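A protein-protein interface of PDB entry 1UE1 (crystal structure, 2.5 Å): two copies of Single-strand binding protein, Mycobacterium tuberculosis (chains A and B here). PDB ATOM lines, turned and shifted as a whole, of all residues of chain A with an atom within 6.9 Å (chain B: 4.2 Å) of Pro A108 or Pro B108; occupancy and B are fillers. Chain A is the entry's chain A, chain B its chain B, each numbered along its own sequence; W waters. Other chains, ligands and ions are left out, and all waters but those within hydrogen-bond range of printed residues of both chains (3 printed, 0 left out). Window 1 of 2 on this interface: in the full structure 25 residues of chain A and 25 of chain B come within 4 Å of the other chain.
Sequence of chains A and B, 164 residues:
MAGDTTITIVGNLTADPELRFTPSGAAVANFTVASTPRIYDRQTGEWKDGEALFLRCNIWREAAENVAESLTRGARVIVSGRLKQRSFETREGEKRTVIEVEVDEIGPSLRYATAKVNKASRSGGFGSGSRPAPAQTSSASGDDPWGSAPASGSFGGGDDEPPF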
ATOM      1  N   SER A  70      -4.913  27.637 -22.085  1.00  0.00           N
ATOM      2  CA  SER A  70      -6.261  27.945 -21.633  1.00  0.00           C
ATOM      3  C   SER A  70      -6.328  28.363 -20.173  1.00  0.00           C
ATOM      4  O   SER A  70      -7.367  28.815 -19.707  1.00  0.00           O
ATOM      5  CB  SER A  70      -7.162  26.732 -21.849  1.00  0.00           C
ATOM      6  OG  SER A  70      -6.905  26.116 -23.100  1.00  0.00           O
ATOM      7  N   LEU A  71      -5.234  28.219 -19.439  1.00  0.00           N
ATOM      8  CA  LEU A  71      -5.265  28.593 -18.029  1.00  0.00           C
ATOM      9  C   LEU A  71      -4.186  29.590 -17.639  1.00  0.00           C
ATOM     10  O   LEU A  71      -3.087  29.599 -18.205  1.00  0.00           O
ATOM     11  CB  LEU A  71      -5.153  27.343 -17.143  1.00  0.00           C
ATOM     12  CG  LEU A  71      -6.248  26.296 -17.309  1.00  0.00           C
ATOM     13  CD1 LEU A  71      -5.967  25.125 -16.418  1.00  0.00           C
ATOM     14  CD2 LEU A  71      -7.575  26.898 -16.980  1.00  0.00           C
ATOM     15  N   ALA A  75      -6.919  30.952 -11.930  1.00  0.00           N
ATOM     16  CA  ALA A  75      -7.969  30.151 -12.541  1.00  0.00           C
ATOM     17  C   ALA A  75      -8.509  29.028 -11.643  1.00  0.00           C
ATOM     18  O   ALA A  75      -7.752  28.217 -11.084  1.00  0.00           O
ATOM     19  CB  ALA A  75      -7.473  29.572 -13.854  1.00  0.00           C
ATOM     20  N   ARG A  76      -9.833  28.990 -11.525  1.00  0.00           N
ATOM     21  CA  ARG A  76     -10.524  27.987 -10.731  1.00  0.00           C
ATOM     22  C   ARG A  76     -10.739  26.766 -11.608  1.00  0.00           C
ATOM     23  O   ARG A  76     -11.482  26.822 -12.588  1.00  0.00           O
ATOM     24  CB  ARG A  76     -11.865  28.523 -10.264  1.00  0.00           C
ATOM     25  CG  ARG A  76     -12.527  27.662  -9.222  1.00  0.00           C
ATOM     26  CD  ARG A  76     -13.942  28.128  -8.946  1.00  0.00           C
ATOM     27  NE  ARG A  76     -14.579  27.320  -7.911  1.00  0.00           N
ATOM     28  CZ  ARG A  76     -14.193  27.293  -6.637  1.00  0.00           C
ATOM     29  NH1 ARG A  76     -13.163  28.028  -6.232  1.00  0.00           N
ATOM     30  NH2 ARG A  76     -14.849  26.546  -5.761  1.00  0.00           N
ATOM     31  N   VAL A  77     -10.102  25.656 -11.241  1.00  0.00           N
ATOM     32  CA  VAL A  77     -10.179  24.442 -12.023  1.00  0.00           C
ATOM     33  C   VAL A  77     -10.755  23.228 -11.308  1.00  0.00           C
ATOM     34  O   VAL A  77     -10.885  23.195 -10.079  1.00  0.00           O
ATOM     35  CB  VAL A  77      -8.777  24.049 -12.525  1.00  0.00           C
ATOM     36  CG1 VAL A  77      -8.263  25.047 -13.563  1.00  0.00           C
ATOM     37  CG2 VAL A  77      -7.825  24.001 -11.349  1.00  0.00           C
ATOM     38  N   ILE A  78     -11.119  22.240 -12.112  1.00  0.00           N
ATOM     39  CA  ILE A  78     -11.616  20.978 -11.611  1.00  0.00           C
ATOM     40  C   ILE A  78     -10.569  20.021 -12.143  1.00  0.00           C
ATOM     41  O   ILE A  78     -10.245  20.045 -13.334  1.00  0.00           O
ATOM     42  CB  ILE A  78     -12.979  20.584 -12.192  1.00  0.00           C
ATOM     43  CG1 ILE A  78     -13.999  21.687 -11.934  1.00  0.00           C
ATOM     44  CG2 ILE A  78     -13.461  19.282 -11.528  1.00  0.00           C
ATOM     45  CD1 ILE A  78     -15.349  21.384 -12.508  1.00  0.00           C
ATOM     46  N   ILE A 106      -8.997  17.832 -16.644  1.00  0.00           N
ATOM     47  CA  ILE A 106      -8.962  19.132 -16.003  1.00  0.00           C
ATOM     48  C   ILE A 106      -9.653  20.093 -16.932  1.00  0.00           C
ATOM     49  O   ILE A 106      -9.574  19.952 -18.156  1.00  0.00           O
ATOM     50  CB  ILE A 106      -7.533  19.648 -15.829  1.00  0.00           C
ATOM     51  CG1 ILE A 106      -7.570  21.049 -15.229  1.00  0.00           C
ATOM     52  CG2 ILE A 106      -6.832  19.691 -17.179  1.00  0.00           C
ATOM     53  CD1 ILE A 106      -6.217  21.610 -14.890  1.00  0.00           C
ATOM     54  N   GLY A 107     -10.314  21.079 -16.348  1.00  0.00           N
ATOM     55  CA  GLY A 107     -11.014  22.066 -17.142  1.00  0.00           C
ATOM     56  C   GLY A 107     -11.355  23.234 -16.253  1.00  0.00           C
ATOM     57  O   GLY A 107     -11.541  23.050 -15.044  1.00  0.00           O
ATOM     58  N   PRO A 108     -11.429  24.452 -16.807  1.00  0.00           N
ATOM     59  CA  PRO A 108     -11.758  25.608 -15.971  1.00  0.00           C
ATOM     60  C   PRO A 108     -13.165  25.457 -15.435  1.00  0.00           C
ATOM     61  O   PRO A 108     -14.057  25.056 -16.165  1.00  0.00           O
ATOM     62  CB  PRO A 108     -11.618  26.780 -16.938  1.00  0.00           C
ATOM     63  CG  PRO A 108     -11.978  26.173 -18.275  1.00  0.00           C
ATOM     64  CD  PRO A 108     -11.245  24.852 -18.215  1.00  0.00           C
ATOM     65  N   SER A 109     -13.359  25.754 -14.155  1.00  0.00           N
ATOM     66  CA  SER A 109     -14.681  25.638 -13.547  1.00  0.00           C
ATOM     67  C   SER A 109     -15.589  26.812 -13.907  1.00  0.00           C
ATOM     68  O   SER A 109     -15.145  27.965 -13.940  1.00  0.00           O
ATOM     69  CB  SER A 109     -14.549  25.547 -12.023  1.00  0.00           C
ATOM     70  OG  SER A 109     -15.797  25.737 -11.375  1.00  0.00           O
ATOM     71  N   LEU A 110     -16.862  26.509 -14.161  1.00  0.00           N
ATOM     72  CA  LEU A 110     -17.854  27.528 -14.504  1.00  0.00           C
ATOM     73  C   LEU A 110     -18.730  27.935 -13.315  1.00  0.00           C
ATOM     74  O   LEU A 110     -19.923  28.170 -13.475  1.00  0.00           O
ATOM     75  CB  LEU A 110     -18.763  27.017 -15.616  1.00  0.00           C
ATOM     76  CG  LEU A 110     -18.134  26.547 -16.923  1.00  0.00           C
ATOM     77  CD1 LEU A 110     -19.250  26.097 -17.826  1.00  0.00           C
ATOM     78  CD2 LEU A 110     -17.331  27.667 -17.581  1.00  0.00           C
ATOM     79  N   ARG A 111     -18.151  28.023 -12.123  1.00  0.00           N
ATOM     80  CA  ARG A 111     -18.930  28.403 -10.951  1.00  0.00           C
ATOM     81  C   ARG A 111     -18.944  29.915 -10.791  1.00  0.00           C
ATOM     82  O   ARG A 111     -19.959  30.493 -10.428  1.00  0.00           O
ATOM     83  CB  ARG A 111     -18.353  27.739  -9.699  1.00  0.00           C
ATOM     84  CG  ARG A 111     -19.152  27.942  -8.428  1.00  0.00           C
ATOM     85  CD  ARG A 111     -18.578  27.060  -7.340  1.00  0.00           C
ATOM     86  NE  ARG A 111     -19.119  27.337  -6.014  1.00  0.00           N
ATOM     87  CZ  ARG A 111     -18.933  26.550  -4.957  1.00  0.00           C
ATOM     88  NH1 ARG A 111     -18.226  25.429  -5.072  1.00  0.00           N
ATOM     89  NH2 ARG A 111     -19.441  26.888  -3.779  1.00  0.00           N
ATOM     90  N   THR A 114     -17.132  32.232 -17.032  1.00  0.00           N
ATOM     91  CA  THR A 114     -17.576  31.657 -18.292  1.00  0.00           C
ATOM     92  C   THR A 114     -16.343  31.378 -19.107  1.00  0.00           C
ATOM     93  O   THR A 114     -15.233  31.712 -18.706  1.00  0.00           O
ATOM     94  CB  THR A 114     -18.500  32.606 -19.105  1.00  0.00           C
ATOM     95  OG1 THR A 114     -17.858  33.877 -19.298  1.00  0.00           O
ATOM     96  CG2 THR A 114     -19.830  32.783 -18.392  1.00  0.00           C
ATOM     97  N   ALA A 115     -16.538  30.751 -20.251  1.00  0.00           N
ATOM     98  CA  ALA A 115     -15.428  30.449 -21.116  1.00  0.00           C
ATOM     99  C   ALA A 115     -15.989  30.103 -22.462  1.00  0.00           C
ATOM    100  O   ALA A 115     -17.091  29.567 -22.558  1.00  0.00           O
ATOM    101  CB  ALA A 115     -14.640  29.278 -20.565  1.00  0.00           C
ATOM    102  N   LYS A 116     -15.247  30.434 -23.506  1.00  0.00           N
ATOM    103  CA  LYS A 116     -15.681  30.086 -24.842  1.00  0.00           C
ATOM    104  C   LYS A 116     -14.881  28.850 -25.202  1.00  0.00           C
ATOM    105  O   LYS A 116     -13.652  28.889 -25.298  1.00  0.00           O
ATOM    106  CB  LYS A 116     -15.428  31.241 -25.810  1.00  0.00           C
ATOM    107  CG  LYS A 116     -16.371  32.411 -25.542  1.00  0.00           C
ATOM    108  CD  LYS A 116     -16.333  33.480 -26.619  1.00  0.00           C
ATOM    109  CE  LYS A 116     -17.364  34.560 -26.323  1.00  0.00           C
ATOM    110  NZ  LYS A 116     -17.363  35.650 -27.335  1.00  0.00           N
ATOM    111  N   VAL A 117     -15.595  27.742 -25.352  1.00  0.00           N
ATOM    112  CA  VAL A 117     -14.985  26.462 -25.671  1.00  0.00           C
ATOM    113  C   VAL A 117     -14.918  26.229 -27.176  1.00  0.00           C
ATOM    114  O   VAL A 117     -15.942  26.039 -27.826  1.00  0.00           O
ATOM    115  CB  VAL A 117     -15.779  25.310 -25.009  1.00  0.00           C
ATOM    116  CG1 VAL A 117     -15.208  23.965 -25.423  1.00  0.00           C
ATOM    117  CG2 VAL A 117     -15.744  25.465 -23.494  1.00  0.00           C
ATOM    118  N   LEU B  71     -21.387  26.309 -22.363  1.00  0.00           N
ATOM    119  CA  LEU B  71     -21.369  24.964 -22.921  1.00  0.00           C
ATOM    120  C   LEU B  71     -22.433  24.624 -23.964  1.00  0.00           C
ATOM    121  O   LEU B  71     -23.586  25.049 -23.872  1.00  0.00           O
ATOM    122  CB  LEU B  71     -21.455  23.957 -21.772  1.00  0.00           C
ATOM    123  CG  LEU B  71     -20.492  24.162 -20.603  1.00  0.00           C
ATOM    124  CD1 LEU B  71     -20.770  23.091 -19.552  1.00  0.00           C
ATOM    125  CD2 LEU B  71     -19.043  24.078 -21.086  1.00  0.00           C
ATOM    126  N   ARG B  76     -17.122  18.212 -24.069  1.00  0.00           N
ATOM    127  CA  ARG B  76     -16.608  17.301 -23.057  1.00  0.00           C
ATOM    128  C   ARG B  76     -16.532  18.121 -21.788  1.00  0.00           C
ATOM    129  O   ARG B  76     -16.028  19.244 -21.804  1.00  0.00           O
ATOM    130  CB  ARG B  76     -15.217  16.795 -23.438  1.00  0.00           C
ATOM    131  CG  ARG B  76     -14.717  15.613 -22.607  1.00  0.00           C
ATOM    132  CD  ARG B  76     -13.569  14.919 -23.325  1.00  0.00           C
ATOM    133  NE  ARG B  76     -13.661  13.470 -23.192  1.00  0.00           N
ATOM    134  CZ  ARG B  76     -13.238  12.790 -22.131  1.00  0.00           C
ATOM    135  NH1 ARG B  76     -13.363  11.471 -22.084  1.00  0.00           N
ATOM    136  NH2 ARG B  76     -12.670  13.431 -21.121  1.00  0.00           N
ATOM    137  N   ILE B 106     -18.514  22.444 -12.480  1.00  0.00           N
ATOM    138  CA  ILE B 106     -18.500  21.850 -13.797  1.00  0.00           C
ATOM    139  C   ILE B 106     -17.681  22.747 -14.684  1.00  0.00           C
ATOM    140  O   ILE B 106     -17.754  23.967 -14.581  1.00  0.00           O
ATOM    141  CB  ILE B 106     -19.903  21.743 -14.377  1.00  0.00           C
ATOM    142  CG1 ILE B 106     -19.828  21.131 -15.777  1.00  0.00           C
ATOM    143  CG2 ILE B 106     -20.560  23.115 -14.397  1.00  0.00           C
ATOM    144  CD1 ILE B 106     -21.166  20.877 -16.418  1.00  0.00           C
ATOM    145  N   GLY B 107     -16.882  22.138 -15.545  1.00  0.00           N
ATOM    146  CA  GLY B 107     -16.049  22.918 -16.431  1.00  0.00           C
ATOM    147  C   GLY B 107     -15.713  22.153 -17.687  1.00  0.00           C
ATOM    148  O   GLY B 107     -15.788  20.924 -17.701  1.00  0.00           O
ATOM    149  N   PRO B 108     -15.372  22.858 -18.775  1.00  0.00           N
ATOM    150  CA  PRO B 108     -15.025  22.192 -20.026  1.00  0.00           C
ATOM    151  C   PRO B 108     -13.673  21.519 -19.886  1.00  0.00           C
ATOM    152  O   PRO B 108     -12.715  22.138 -19.446  1.00  0.00           O
ATOM    153  CB  PRO B 108     -14.986  23.341 -21.019  1.00  0.00           C
ATOM    154  CG  PRO B 108     -14.553  24.482 -20.172  1.00  0.00           C
ATOM    155  CD  PRO B 108     -15.439  24.311 -18.981  1.00  0.00           C
ATOM    156  N   SER B 109     -13.597  20.248 -20.251  1.00  0.00           N
ATOM    157  CA  SER B 109     -12.334  19.535 -20.161  1.00  0.00           C
ATOM    158  C   SER B 109     -11.398  19.993 -21.270  1.00  0.00           C
ATOM    159  O   SER B 109     -11.763  20.001 -22.446  1.00  0.00           O
ATOM    160  CB  SER B 109     -12.565  18.031 -20.276  1.00  0.00           C
ATOM    161  OG  SER B 109     -11.367  17.374 -20.624  1.00  0.00           O
ATOM    162  N   LEU B 110     -10.190  20.376 -20.879  1.00  0.00           N
ATOM    163  CA  LEU B 110      -9.173  20.821 -21.815  1.00  0.00           C
ATOM    164  C   LEU B 110      -8.447  19.634 -22.424  1.00  0.00           C
ATOM    165  O   LEU B 110      -7.276  19.739 -22.780  1.00  0.00           O
ATOM    166  CB  LEU B 110      -8.166  21.709 -21.105  1.00  0.00           C
ATOM    167  CG  LEU B 110      -8.749  23.010 -20.587  1.00  0.00           C
ATOM    168  CD1 LEU B 110      -7.684  23.779 -19.860  1.00  0.00           C
ATOM    169  CD2 LEU B 110      -9.297  23.813 -21.757  1.00  0.00           C
ATOM    170  N   VAL B 117     -11.209  31.638 -20.595  1.00  0.00           N
ATOM    171  CA  VAL B 117     -11.947  31.834 -19.361  1.00  0.00           C
ATOM    172  C   VAL B 117     -11.988  33.273 -18.879  1.00  0.00           C
ATOM    173  O   VAL B 117     -10.943  33.863 -18.616  1.00  0.00           O
ATOM    174  CB  VAL B 117     -11.342  30.959 -18.232  1.00  0.00           C
ATOM    175  CG1 VAL B 117     -12.252  30.966 -17.013  1.00  0.00           C
ATOM    176  CG2 VAL B 117     -11.122  29.537 -18.733  1.00  0.00           C
HETATM  177  O   HOH W   1      -8.884  17.207 -19.120  1.00  0.00           O
HETATM  178  O   HOH W   2      -7.962  31.700 -20.173  1.00  0.00           O
HETATM  179  O   HOH W   3     -19.364  25.498 -11.605  1.00  0.00           O
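Of chain B, only Gly B107, Pro B108, Leu B110 and Val B117 come within 4 Å of Pro A108.
Pro B108 touches just these residues of chain A: Gly A107 (2.9 Å), Pro A108 (3.2 Å) and Val A117 (3.3 Å).
Printed residues of chain B within 4 Å of Ile A78: Ile B106 and Gly B107.
Of the printed residues of chain A, Leu B71 touches Leu A110.
Printed residues of chain B within 4 Å of Ala A115: Val B117.
Of the printed residues of chain A, Val B117 touches Ser A70 (3.9 Å), Pro A108 (3.3 Å), Thr A114 (3.4 Å) and Ala A115 (3.9 Å).
Ala A75 touches none of the printed residues of chain B.
Arg B76 touches none of the printed residues of chain A.
Water W1 lies within hydrogen-bond range of N of Ile A106 and OG of Ser B109.
Water W3 lies within hydrogen-bond range of N of Arg A111 (2.8 Å), N of Ile B106 (3.3 Å) and O of Leu A110 (3.3 Å).
Water W2 bridges the backbone carbonyl oxygen (O) of Ser A70 (3.0 Å) and the backbone NH (N) of Val B117 (3.3 Å).
Hydrophobic or aromatic side chains of chain A within 4 Å of the printed part of chain B: Leu A71, Ile A78, Pro A108, Leu A110, Ala A115 and Val A117.
CD2 of Leu B110 touches OG of Ser A70, at 3.6 Å.
Ser A70 touches Val B117.
Leu A71 touches Leu B110.
Ile A78 touches Ile B106.
N of Gly B107 touches CD1 of Ile A78 (3.5 Å).
Ile A106 touches Ser B109.
Pro B108 touches Gly A107 (O to CA, 2.9 Å).
CA of Gly B107 touches O of Pro A108 (2.9 Å).
CG2 of Val B117 touches CB of Pro A108, 3.3 Å away.
C of Ser A109 touches O of Ile B106 (3.6 Å).
The backbone carbonyl oxygen (O) of Arg A76 sits at hydrogen-bond distance from the backbone NH (N) of Ser A109 (2.7 Å).
The backbone NH (N) of Ile A78 sits at hydrogen-bond distance from the backbone carbonyl oxygen (O) of Gly A107.
The side-chain hydroxyl of Ser A109 lies close to the backbone NH of Arg A111, at 3.4 Å.
O of Arg B76 sits at hydrogen-bond distance from N of Ser B109, 3.1 Å away.
Ile A106 touches Ser B109, and with the chains exchanged Ser A109 touches Ile B106.
Ile A106 touches Leu B110, and with the chains exchanged Leu A110 touches Ile B106.
Gly A107 touches Pro B108, and with the chains exchanged Pro A108 touches Gly B107.
Pro A108 touches its own counterpart, Pro B108.
Of the 18 pairs that touch across the chains among the printed residues, 11 have their exchanged pair printed and touching as well.
O of Ile A106 lies within hydrogen-bond range of N of Leu B110 (2.8 Å).
The backbone NH (N) of Leu A110 lies within hydrogen-bond range of the backbone carbonyl oxygen (O) of Ile B106 (2.7 Å).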
